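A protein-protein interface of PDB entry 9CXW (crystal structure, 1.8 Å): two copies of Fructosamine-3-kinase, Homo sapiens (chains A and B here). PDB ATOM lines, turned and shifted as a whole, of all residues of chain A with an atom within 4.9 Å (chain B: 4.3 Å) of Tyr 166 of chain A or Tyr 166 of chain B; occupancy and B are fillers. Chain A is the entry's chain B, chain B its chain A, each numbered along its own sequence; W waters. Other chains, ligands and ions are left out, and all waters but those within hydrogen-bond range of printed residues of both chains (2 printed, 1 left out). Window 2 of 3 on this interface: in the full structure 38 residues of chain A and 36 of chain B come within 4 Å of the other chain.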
ATOM      1  N   LEU A 161      10.138  26.344   9.255  1.00  0.00           N
ATOM      2  CA  LEU A 161      11.129  26.893  10.193  1.00  0.00           C
ATOM      3  C   LEU A 161      11.268  26.028  11.431  1.00  0.00           C
ATOM      4  O   LEU A 161      12.381  25.804  11.922  1.00  0.00           O
ATOM      5  CB  LEU A 161      10.715  28.317  10.603  1.00  0.00           C
ATOM      6  CG  LEU A 161      11.761  29.328  11.000  1.00  0.00           C
ATOM      7  CD1 LEU A 161      12.889  29.372   9.987  1.00  0.00           C
ATOM      8  CD2 LEU A 161      11.013  30.700  11.080  1.00  0.00           C
ATOM      9  N   ILE A 162      10.163  25.502  11.937  1.00  0.00           N
ATOM     10  CA  ILE A 162      10.270  24.590  13.072  1.00  0.00           C
ATOM     11  C   ILE A 162      11.043  23.337  12.685  1.00  0.00           C
ATOM     12  O   ILE A 162      11.884  22.854  13.460  1.00  0.00           O
ATOM     13  CB  ILE A 162       8.879  24.267  13.628  1.00  0.00           C
ATOM     14  CG1 ILE A 162       8.423  25.452  14.490  1.00  0.00           C
ATOM     15  CG2 ILE A 162       8.898  23.025  14.534  1.00  0.00           C
ATOM     16  CD1 ILE A 162       6.912  25.573  14.508  1.00  0.00           C
ATOM     17  N   GLU A 163      10.817  22.814  11.473  1.00  0.00           N
ATOM     18  CA  GLU A 163      11.602  21.649  11.036  1.00  0.00           C
ATOM     19  C   GLU A 163      13.071  22.004  10.935  1.00  0.00           C
ATOM     20  O   GLU A 163      13.946  21.242  11.375  1.00  0.00           O
ATOM     21  CB  GLU A 163      11.109  21.131   9.682  1.00  0.00           C
ATOM     22  CG  GLU A 163      11.969  19.909   9.133  1.00  0.00           C
ATOM     23  CD  GLU A 163      11.953  18.714  10.081  1.00  0.00           C
ATOM     24  OE1 GLU A 163      10.976  18.495  10.813  1.00  0.00           O
ATOM     25  OE2 GLU A 163      12.894  17.912  10.057  1.00  0.00           O
ATOM     26  N   LYS A 164      13.370  23.114  10.280  1.00  0.00           N
ATOM     27  CA  LYS A 164      14.765  23.501  10.107  1.00  0.00           C
ATOM     28  C   LYS A 164      15.476  23.645  11.459  1.00  0.00           C
ATOM     29  O   LYS A 164      16.575  23.103  11.671  1.00  0.00           O
ATOM     30  CB  LYS A 164      14.835  24.794   9.307  1.00  0.00           C
ATOM     31  CG  LYS A 164      16.204  25.458   9.356  1.00  0.00           C
ATOM     32  CD  LYS A 164      16.449  26.447   8.219  1.00  0.00           C
ATOM     33  CE  LYS A 164      15.764  27.773   8.482  1.00  0.00           C
ATOM     34  NZ  LYS A 164      16.548  28.652   9.427  1.00  0.00           N
ATOM     35  N   ASP A 165      14.862  24.369  12.385  1.00  0.00           N
ATOM     36  CA  ASP A 165      15.586  24.767  13.590  1.00  0.00           C
ATOM     37  C   ASP A 165      15.424  23.820  14.765  1.00  0.00           C
ATOM     38  O   ASP A 165      16.341  23.733  15.597  1.00  0.00           O
ATOM     39  CB  ASP A 165      15.127  26.157  14.049  1.00  0.00           C
ATOM     40  CG  ASP A 165      15.513  27.240  13.095  1.00  0.00           C
ATOM     41  OD1 ASP A 165      16.408  26.998  12.255  1.00  0.00           O
ATOM     42  OD2 ASP A 165      14.954  28.362  13.220  1.00  0.00           O
ATOM     43  N   TYR A 166      14.308  23.096  14.848  1.00  0.00           N
ATOM     44  CA  TYR A 166      14.016  22.207  15.961  1.00  0.00           C
ATOM     45  C   TYR A 166      13.864  20.759  15.544  1.00  0.00           C
ATOM     46  O   TYR A 166      13.847  19.893  16.418  1.00  0.00           O
ATOM     47  CB  TYR A 166      12.742  22.642  16.712  1.00  0.00           C
ATOM     48  CG  TYR A 166      12.770  24.084  17.254  1.00  0.00           C
ATOM     49  CD1 TYR A 166      13.396  24.404  18.468  1.00  0.00           C
ATOM     50  CD2 TYR A 166      12.095  25.090  16.605  1.00  0.00           C
ATOM     51  CE1 TYR A 166      13.398  25.744  18.970  1.00  0.00           C
ATOM     52  CE2 TYR A 166      12.078  26.424  17.092  1.00  0.00           C
ATOM     53  CZ  TYR A 166      12.742  26.743  18.287  1.00  0.00           C
ATOM     54  OH  TYR A 166      12.716  28.063  18.774  1.00  0.00           O
ATOM     55  N   ALA A 167      13.696  20.478  14.247  1.00  0.00           N
ATOM     56  CA  ALA A 167      13.564  19.100  13.745  1.00  0.00           C
ATOM     57  C   ALA A 167      12.585  18.288  14.587  1.00  0.00           C
ATOM     58  O   ALA A 167      12.847  17.143  14.972  1.00  0.00           O
ATOM     59  CB  ALA A 167      14.930  18.416  13.687  1.00  0.00           C
ATOM     60  N   ASP A 168      11.424  18.882  14.845  1.00  0.00           N
ATOM     61  CA  ASP A 168      10.443  18.317  15.762  1.00  0.00           C
ATOM     62  C   ASP A 168       9.574  17.275  15.071  1.00  0.00           C
ATOM     63  O   ASP A 168       8.721  17.616  14.237  1.00  0.00           O
ATOM     64  CB  ASP A 168       9.555  19.419  16.346  1.00  0.00           C
ATOM     65  CG  ASP A 168       8.851  18.945  17.579  1.00  0.00           C
ATOM     66  OD1 ASP A 168       9.336  19.171  18.694  1.00  0.00           O
ATOM     67  OD2 ASP A 168       7.773  18.343  17.445  1.00  0.00           O
ATOM     68  N   TRP A 271       6.804  29.967  19.090  1.00  0.00           N
ATOM     69  CA  TRP A 271       7.843  28.927  19.164  1.00  0.00           C
ATOM     70  C   TRP A 271       9.080  29.332  18.367  1.00  0.00           C
ATOM     71  O   TRP A 271      10.222  29.226  18.853  1.00  0.00           O
ATOM     72  CB  TRP A 271       7.243  27.620  18.660  1.00  0.00           C
ATOM     73  CG  TRP A 271       8.104  26.349  18.827  1.00  0.00           C
ATOM     74  CD1 TRP A 271       9.387  26.247  19.325  1.00  0.00           C
ATOM     75  CD2 TRP A 271       7.678  25.019  18.516  1.00  0.00           C
ATOM     76  NE1 TRP A 271       9.799  24.896  19.307  1.00  0.00           N
ATOM     77  CE2 TRP A 271       8.753  24.140  18.812  1.00  0.00           C
ATOM     78  CE3 TRP A 271       6.483  24.479  17.973  1.00  0.00           C
ATOM     79  CZ2 TRP A 271       8.667  22.746  18.586  1.00  0.00           C
ATOM     80  CZ3 TRP A 271       6.404  23.096  17.747  1.00  0.00           C
ATOM     81  CH2 TRP A 271       7.487  22.245  18.068  1.00  0.00           C
ATOM     82  N   ASN A 272       8.880  29.823  17.143  1.00  0.00           N
ATOM     83  CA  ASN A 272      10.006  30.288  16.336  1.00  0.00           C
ATOM     84  C   ASN A 272      10.684  31.524  16.941  1.00  0.00           C
ATOM     85  O   ASN A 272      11.926  31.598  16.972  1.00  0.00           O
ATOM     86  CB  ASN A 272       9.558  30.565  14.911  1.00  0.00           C
ATOM     87  CG  ASN A 272       9.490  29.260  14.086  1.00  0.00           C
ATOM     88  OD1 ASN A 272      10.414  28.420  14.183  1.00  0.00           O
ATOM     89  ND2 ASN A 272       8.366  29.032  13.378  1.00  0.00           N
ATOM     90  N   GLY A 275      11.091  30.294  21.417  1.00  0.00           N
ATOM     91  CA  GLY A 275      11.638  28.985  21.768  1.00  0.00           C
ATOM     92  C   GLY A 275      10.672  27.972  22.348  1.00  0.00           C
ATOM     93  O   GLY A 275       9.444  28.066  22.251  1.00  0.00           O
ATOM     94  N   ARG A 276      11.267  26.970  22.993  1.00  0.00           N
ATOM     95  CA  ARG A 276      10.614  25.693  23.276  1.00  0.00           C
ATOM     96  C   ARG A 276       9.460  25.807  24.246  1.00  0.00           C
ATOM     97  O   ARG A 276       8.633  24.884  24.308  1.00  0.00           O
ATOM     98  CB  ARG A 276      11.640  24.712  23.904  1.00  0.00           C
ATOM     99  CG  ARG A 276      12.141  25.248  25.303  1.00  0.00           C
ATOM    100  CD  ARG A 276      13.279  24.412  25.983  1.00  0.00           C
ATOM    101  NE  ARG A 276      12.849  23.085  26.425  1.00  0.00           N
ATOM    102  CZ  ARG A 276      13.337  21.929  25.973  1.00  0.00           C
ATOM    103  NH1 ARG A 276      14.282  21.889  25.045  1.00  0.00           N
ATOM    104  NH2 ARG A 276      12.900  20.786  26.507  1.00  0.00           N
ATOM    105  N   ILE B 162      20.059  17.340  24.106  1.00  0.00           N
ATOM    106  CA  ILE B 162      20.428  17.445  22.700  1.00  0.00           C
ATOM    107  C   ILE B 162      20.470  16.080  22.027  1.00  0.00           C
ATOM    108  O   ILE B 162      20.066  15.945  20.867  1.00  0.00           O
ATOM    109  CB  ILE B 162      21.733  18.235  22.505  1.00  0.00           C
ATOM    110  CG1 ILE B 162      21.515  19.707  22.841  1.00  0.00           C
ATOM    111  CG2 ILE B 162      22.323  18.022  21.123  1.00  0.00           C
ATOM    112  CD1 ILE B 162      22.839  20.409  23.095  1.00  0.00           C
ATOM    113  N   GLU B 163      20.939  15.052  22.732  1.00  0.00           N
ATOM    114  CA  GLU B 163      20.878  13.717  22.150  1.00  0.00           C
ATOM    115  C   GLU B 163      19.425  13.294  21.908  1.00  0.00           C
ATOM    116  O   GLU B 163      19.080  12.815  20.823  1.00  0.00           O
ATOM    117  CB  GLU B 163      21.605  12.721  23.048  1.00  0.00           C
ATOM    118  CG  GLU B 163      21.570  11.274  22.530  1.00  0.00           C
ATOM    119  CD  GLU B 163      22.221  11.066  21.158  1.00  0.00           C
ATOM    120  OE1 GLU B 163      23.084  11.848  20.720  1.00  0.00           O
ATOM    121  OE2 GLU B 163      21.853  10.082  20.490  1.00  0.00           O
ATOM    122  N   LYS B 164      18.566  13.466  22.911  1.00  0.00           N
ATOM    123  CA  LYS B 164      17.159  13.108  22.766  1.00  0.00           C
ATOM    124  C   LYS B 164      16.509  13.810  21.575  1.00  0.00           C
ATOM    125  O   LYS B 164      15.867  13.173  20.730  1.00  0.00           O
ATOM    126  CB  LYS B 164      16.401  13.485  24.035  1.00  0.00           C
ATOM    127  CG  LYS B 164      15.044  12.830  24.074  1.00  0.00           C
ATOM    128  CD  LYS B 164      14.557  12.666  25.470  1.00  0.00           C
ATOM    129  CE  LYS B 164      13.895  13.958  25.924  1.00  0.00           C
ATOM    130  NZ  LYS B 164      13.036  13.737  27.132  1.00  0.00           N
ATOM    131  N   ASP B 165      16.655  15.131  21.495  1.00  0.00           N
ATOM    132  CA  ASP B 165      15.843  15.900  20.561  1.00  0.00           C
ATOM    133  C   ASP B 165      16.510  16.092  19.212  1.00  0.00           C
ATOM    134  O   ASP B 165      15.818  16.403  18.244  1.00  0.00           O
ATOM    135  CB  ASP B 165      15.456  17.265  21.164  1.00  0.00           C
ATOM    136  CG  ASP B 165      14.602  17.127  22.405  1.00  0.00           C
ATOM    137  OD1 ASP B 165      13.892  16.100  22.536  1.00  0.00           O
ATOM    138  OD2 ASP B 165      14.638  18.039  23.268  1.00  0.00           O
ATOM    139  N   TYR B 166      17.831  15.969  19.120  1.00  0.00           N
ATOM    140  CA  TYR B 166      18.530  16.199  17.864  1.00  0.00           C
ATOM    141  C   TYR B 166      19.383  15.038  17.414  1.00  0.00           C
ATOM    142  O   TYR B 166      19.789  15.029  16.246  1.00  0.00           O
ATOM    143  CB  TYR B 166      19.443  17.437  17.947  1.00  0.00           C
ATOM    144  CG  TYR B 166      18.692  18.717  18.193  1.00  0.00           C
ATOM    145  CD1 TYR B 166      18.163  19.458  17.125  1.00  0.00           C
ATOM    146  CD2 TYR B 166      18.443  19.154  19.494  1.00  0.00           C
ATOM    147  CE1 TYR B 166      17.432  20.621  17.352  1.00  0.00           C
ATOM    148  CE2 TYR B 166      17.711  20.331  19.739  1.00  0.00           C
ATOM    149  CZ  TYR B 166      17.206  21.046  18.645  1.00  0.00           C
ATOM    150  OH  TYR B 166      16.487  22.193  18.868  1.00  0.00           O
ATOM    151  N   ALA B 167      19.704  14.085  18.297  1.00  0.00           N
ATOM    152  CA  ALA B 167      20.580  12.949  17.961  1.00  0.00           C
ATOM    153  C   ALA B 167      21.833  13.422  17.226  1.00  0.00           C
ATOM    154  O   ALA B 167      22.204  12.904  16.169  1.00  0.00           O
ATOM    155  CB  ALA B 167      19.835  11.893  17.141  1.00  0.00           C
ATOM    156  N   ASP B 168      22.486  14.444  17.784  1.00  0.00           N
ATOM    157  CA  ASP B 168      23.606  15.083  17.096  1.00  0.00           C
ATOM    158  C   ASP B 168      24.874  14.279  17.341  1.00  0.00           C
ATOM    159  O   ASP B 168      25.354  14.202  18.479  1.00  0.00           O
ATOM    160  CB  ASP B 168      23.779  16.531  17.549  1.00  0.00           C
ATOM    161  CG  ASP B 168      24.669  17.313  16.614  1.00  0.00           C
ATOM    162  OD1 ASP B 168      24.164  18.063  15.755  1.00  0.00           O
ATOM    163  OD2 ASP B 168      25.899  17.193  16.743  1.00  0.00           O
ATOM    164  N   TRP B 271      20.800  26.284  22.465  1.00  0.00           N
ATOM    165  CA  TRP B 271      20.433  25.265  21.473  1.00  0.00           C
ATOM    166  C   TRP B 271      19.160  24.539  21.900  1.00  0.00           C
ATOM    167  O   TRP B 271      18.209  24.427  21.113  1.00  0.00           O
ATOM    168  CB  TRP B 271      21.622  24.296  21.265  1.00  0.00           C
ATOM    169  CG  TRP B 271      21.492  23.215  20.196  1.00  0.00           C
ATOM    170  CD1 TRP B 271      20.374  22.901  19.433  1.00  0.00           C
ATOM    171  CD2 TRP B 271      22.512  22.284  19.816  1.00  0.00           C
ATOM    172  NE1 TRP B 271      20.663  21.835  18.588  1.00  0.00           N
ATOM    173  CE2 TRP B 271      21.966  21.441  18.806  1.00  0.00           C
ATOM    174  CE3 TRP B 271      23.856  22.070  20.235  1.00  0.00           C
ATOM    175  CZ2 TRP B 271      22.705  20.401  18.228  1.00  0.00           C
ATOM    176  CZ3 TRP B 271      24.574  21.038  19.670  1.00  0.00           C
ATOM    177  CH2 TRP B 271      23.999  20.209  18.662  1.00  0.00           C
ATOM    178  N   HIS B 273      16.848  25.680  23.925  1.00  0.00           N
ATOM    179  CA  HIS B 273      15.710  26.620  23.930  1.00  0.00           C
ATOM    180  C   HIS B 273      15.281  27.081  22.536  1.00  0.00           C
ATOM    181  O   HIS B 273      14.081  27.217  22.269  1.00  0.00           O
ATOM    182  CB  HIS B 273      16.040  27.849  24.771  1.00  0.00           C
ATOM    183  CG  HIS B 273      15.778  27.657  26.234  1.00  0.00           C
ATOM    184  ND1 HIS B 273      16.691  27.051  27.081  1.00  0.00           N
ATOM    185  CD2 HIS B 273      14.723  28.006  27.005  1.00  0.00           C
ATOM    186  CE1 HIS B 273      16.203  27.039  28.310  1.00  0.00           C
ATOM    187  NE2 HIS B 273      15.001  27.595  28.286  1.00  0.00           N
ATOM    188  N   PHE B 274      16.227  27.434  21.679  1.00  0.00           N
ATOM    189  CA  PHE B 274      15.982  28.155  20.440  1.00  0.00           C
ATOM    190  C   PHE B 274      16.366  27.378  19.187  1.00  0.00           C
ATOM    191  O   PHE B 274      16.119  27.877  18.084  1.00  0.00           O
ATOM    192  CB  PHE B 274      16.741  29.491  20.452  1.00  0.00           C
ATOM    193  CG  PHE B 274      16.446  30.312  21.664  1.00  0.00           C
ATOM    194  CD1 PHE B 274      15.167  30.848  21.857  1.00  0.00           C
ATOM    195  CD2 PHE B 274      17.401  30.483  22.662  1.00  0.00           C
ATOM    196  CE1 PHE B 274      14.862  31.572  22.987  1.00  0.00           C
ATOM    197  CE2 PHE B 274      17.107  31.216  23.797  1.00  0.00           C
ATOM    198  CZ  PHE B 274      15.833  31.759  23.973  1.00  0.00           C
ATOM    199  N   GLY B 275      16.991  26.200  19.323  1.00  0.00           N
ATOM    200  CA  GLY B 275      17.268  25.326  18.193  1.00  0.00           C
ATOM    201  C   GLY B 275      18.644  25.513  17.581  1.00  0.00           C
ATOM    202  O   GLY B 275      19.566  26.067  18.178  1.00  0.00           O
ATOM    203  N   ARG B 276      18.771  25.029  16.343  1.00  0.00           N
ATOM    204  CA  ARG B 276      20.048  24.785  15.687  1.00  0.00           C
ATOM    205  C   ARG B 276      20.844  26.039  15.339  1.00  0.00           C
ATOM    206  O   ARG B 276      22.012  25.900  14.949  1.00  0.00           O
ATOM    207  CB  ARG B 276      19.822  23.926  14.441  1.00  0.00           C
ATOM    208  CG  ARG B 276      19.573  22.460  14.810  1.00  0.00           C
ATOM    209  CD  ARG B 276      19.315  21.612  13.544  1.00  0.00           C
ATOM    210  NE  ARG B 276      20.525  20.887  13.171  1.00  0.00           N
ATOM    211  CZ  ARG B 276      21.377  21.288  12.235  1.00  0.00           C
ATOM    212  NH1 ARG B 276      21.183  22.410  11.554  1.00  0.00           N
ATOM    213  NH2 ARG B 276      22.466  20.562  11.995  1.00  0.00           N
HETATM  214  O   HOH W   1      15.948  20.252  23.193  1.00  0.00           O
HETATM  215  O   HOH W   2      14.305  29.874  16.965  1.00  0.00           O
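The backbone carbonyl oxygen of His 273 of chain B sits at hydrogen-bond distance from the backbone NH of Arg 276 of chain A, 2.9 Å away.
O of Phe 274 of chain B is in hydrogen-bond range of OH of Tyr 166 of chain A, at 3.5 Å.
The backbone carbonyl oxygen (O) of Asp 165 of chain A is in hydrogen-bond range of the backbone NH (N) of Arg 276 of chain B (2.9 Å).
The side-chain carboxylate of Asp 165 of chain A lies within salt-bridge range of the side-chain amino group of Lys 164 of chain A, 3.3 Å away.
The side-chain hydroxyl (OH) of Tyr 166 of chain A sits at hydrogen-bond distance from the backbone carbonyl oxygen (O) of Trp 271 of chain A.
Among the printed residues, pairs that only touch across the chains: Lys 164 of chain A with Arg 276 of chain B (3.6 Å), Asp 165 of chain A with Tyr 166 of chain B (3.6 Å), Asp 165 of chain A with Gly 275 of chain B (3.2 Å), Tyr 166 of chain A with Tyr 166 of chain B (3.8 Å), Tyr 166 of chain A with His 273 of chain B (3.7 Å), Tyr 166 of chain A with Gly 275 of chain B (3.6 Å), Gly 275 of chain A with His 273 of chain B (3.1 Å) and Gly 275 of chain A with Phe 274 of chain B (3.99 Å).
Of chain A, only Asp 165 (3.6 Å) and Tyr 166 (3.8 Å) come within 4 Å of Tyr 166 of chain B.
Printed residues of chain A within 4 Å of Gly 275 of chain B: Asp 165 (3.2 Å) and Tyr 166 (3.6 Å).
Of the printed residues of chain B, Lys 164 of chain A touches Arg 276.
Of the printed residues of chain B, Arg 276 of chain A touches His 273.
Of the printed residues of chain A, Arg 276 of chain B touches Lys 164 (3.6 Å) and Asp 165 (2.9 Å).
Of the printed residues of chain A, His 273 of chain B touches Tyr 166 (3.7 Å), Gly 275 (3.1 Å) and Arg 276 (2.9 Å).
Ile 162 of chain B touches none of the printed residues of chain A.
The nearest printed residue of chain B that does not touch Tyr 166 of chain A is Asp 165 of chain B (4.4 Å).
Along chain A the printed residues that touch a printed residue of chain B span positions 164 to 276.
Of the 12 printed residues of chain B, 5 touch a printed residue of chain A.
Printed residues of chain B that touch a printed residue of chain A: Tyr 166, His 273, Phe 274, Gly 275 and Arg 276.
Hydrophobic or aromatic side chains of chain B within 4 Å of the printed part of chain A: Tyr 166 and Phe 274.
Among the printed residues, no Asp or Glu carboxylate lies within 4 Å of a Lys or Arg side-chain nitrogen of the other chain.
Lys 164 of chain A touches Arg 276 of chain B, but with the chains exchanged Arg 276 of chain A does not touch Lys 164 of chain B (6.9 Å).
Asp 165 of chain A touches Tyr 166 of chain B, but with the chains exchanged Tyr 166 of chain A does not touch Asp 165 of chain B (4.4 Å).
Asp 165 of chain A touches Gly 275 of chain B, but with the chains exchanged Gly 275 of chain A does not touch Asp 165 of chain B (10.7 Å).
Tyr 166 of chain B touches its own counterpart, Tyr 166 of chain A.
Positions printed for both chains: 162, 163, 164, 165, 166, 167, 168, 271, 275 and 276.
Of the 11 pairs that touch across the chains among the printed residues, 1 has its exchanged pair printed and touching as well.
Water W1 bridges OD2 of Asp 165 of chain B (2.6 Å) and NH1 of Arg 276 of chain A (3.0 Å).
Water W2 lies within hydrogen-bond range of the backbone carbonyl oxygen (O) of Phe 274 of chain B, the backbone carbonyl oxygen (O) of Asn 272 of chain A and the side-chain hydroxyl (OH) of Tyr 166 of chain A.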
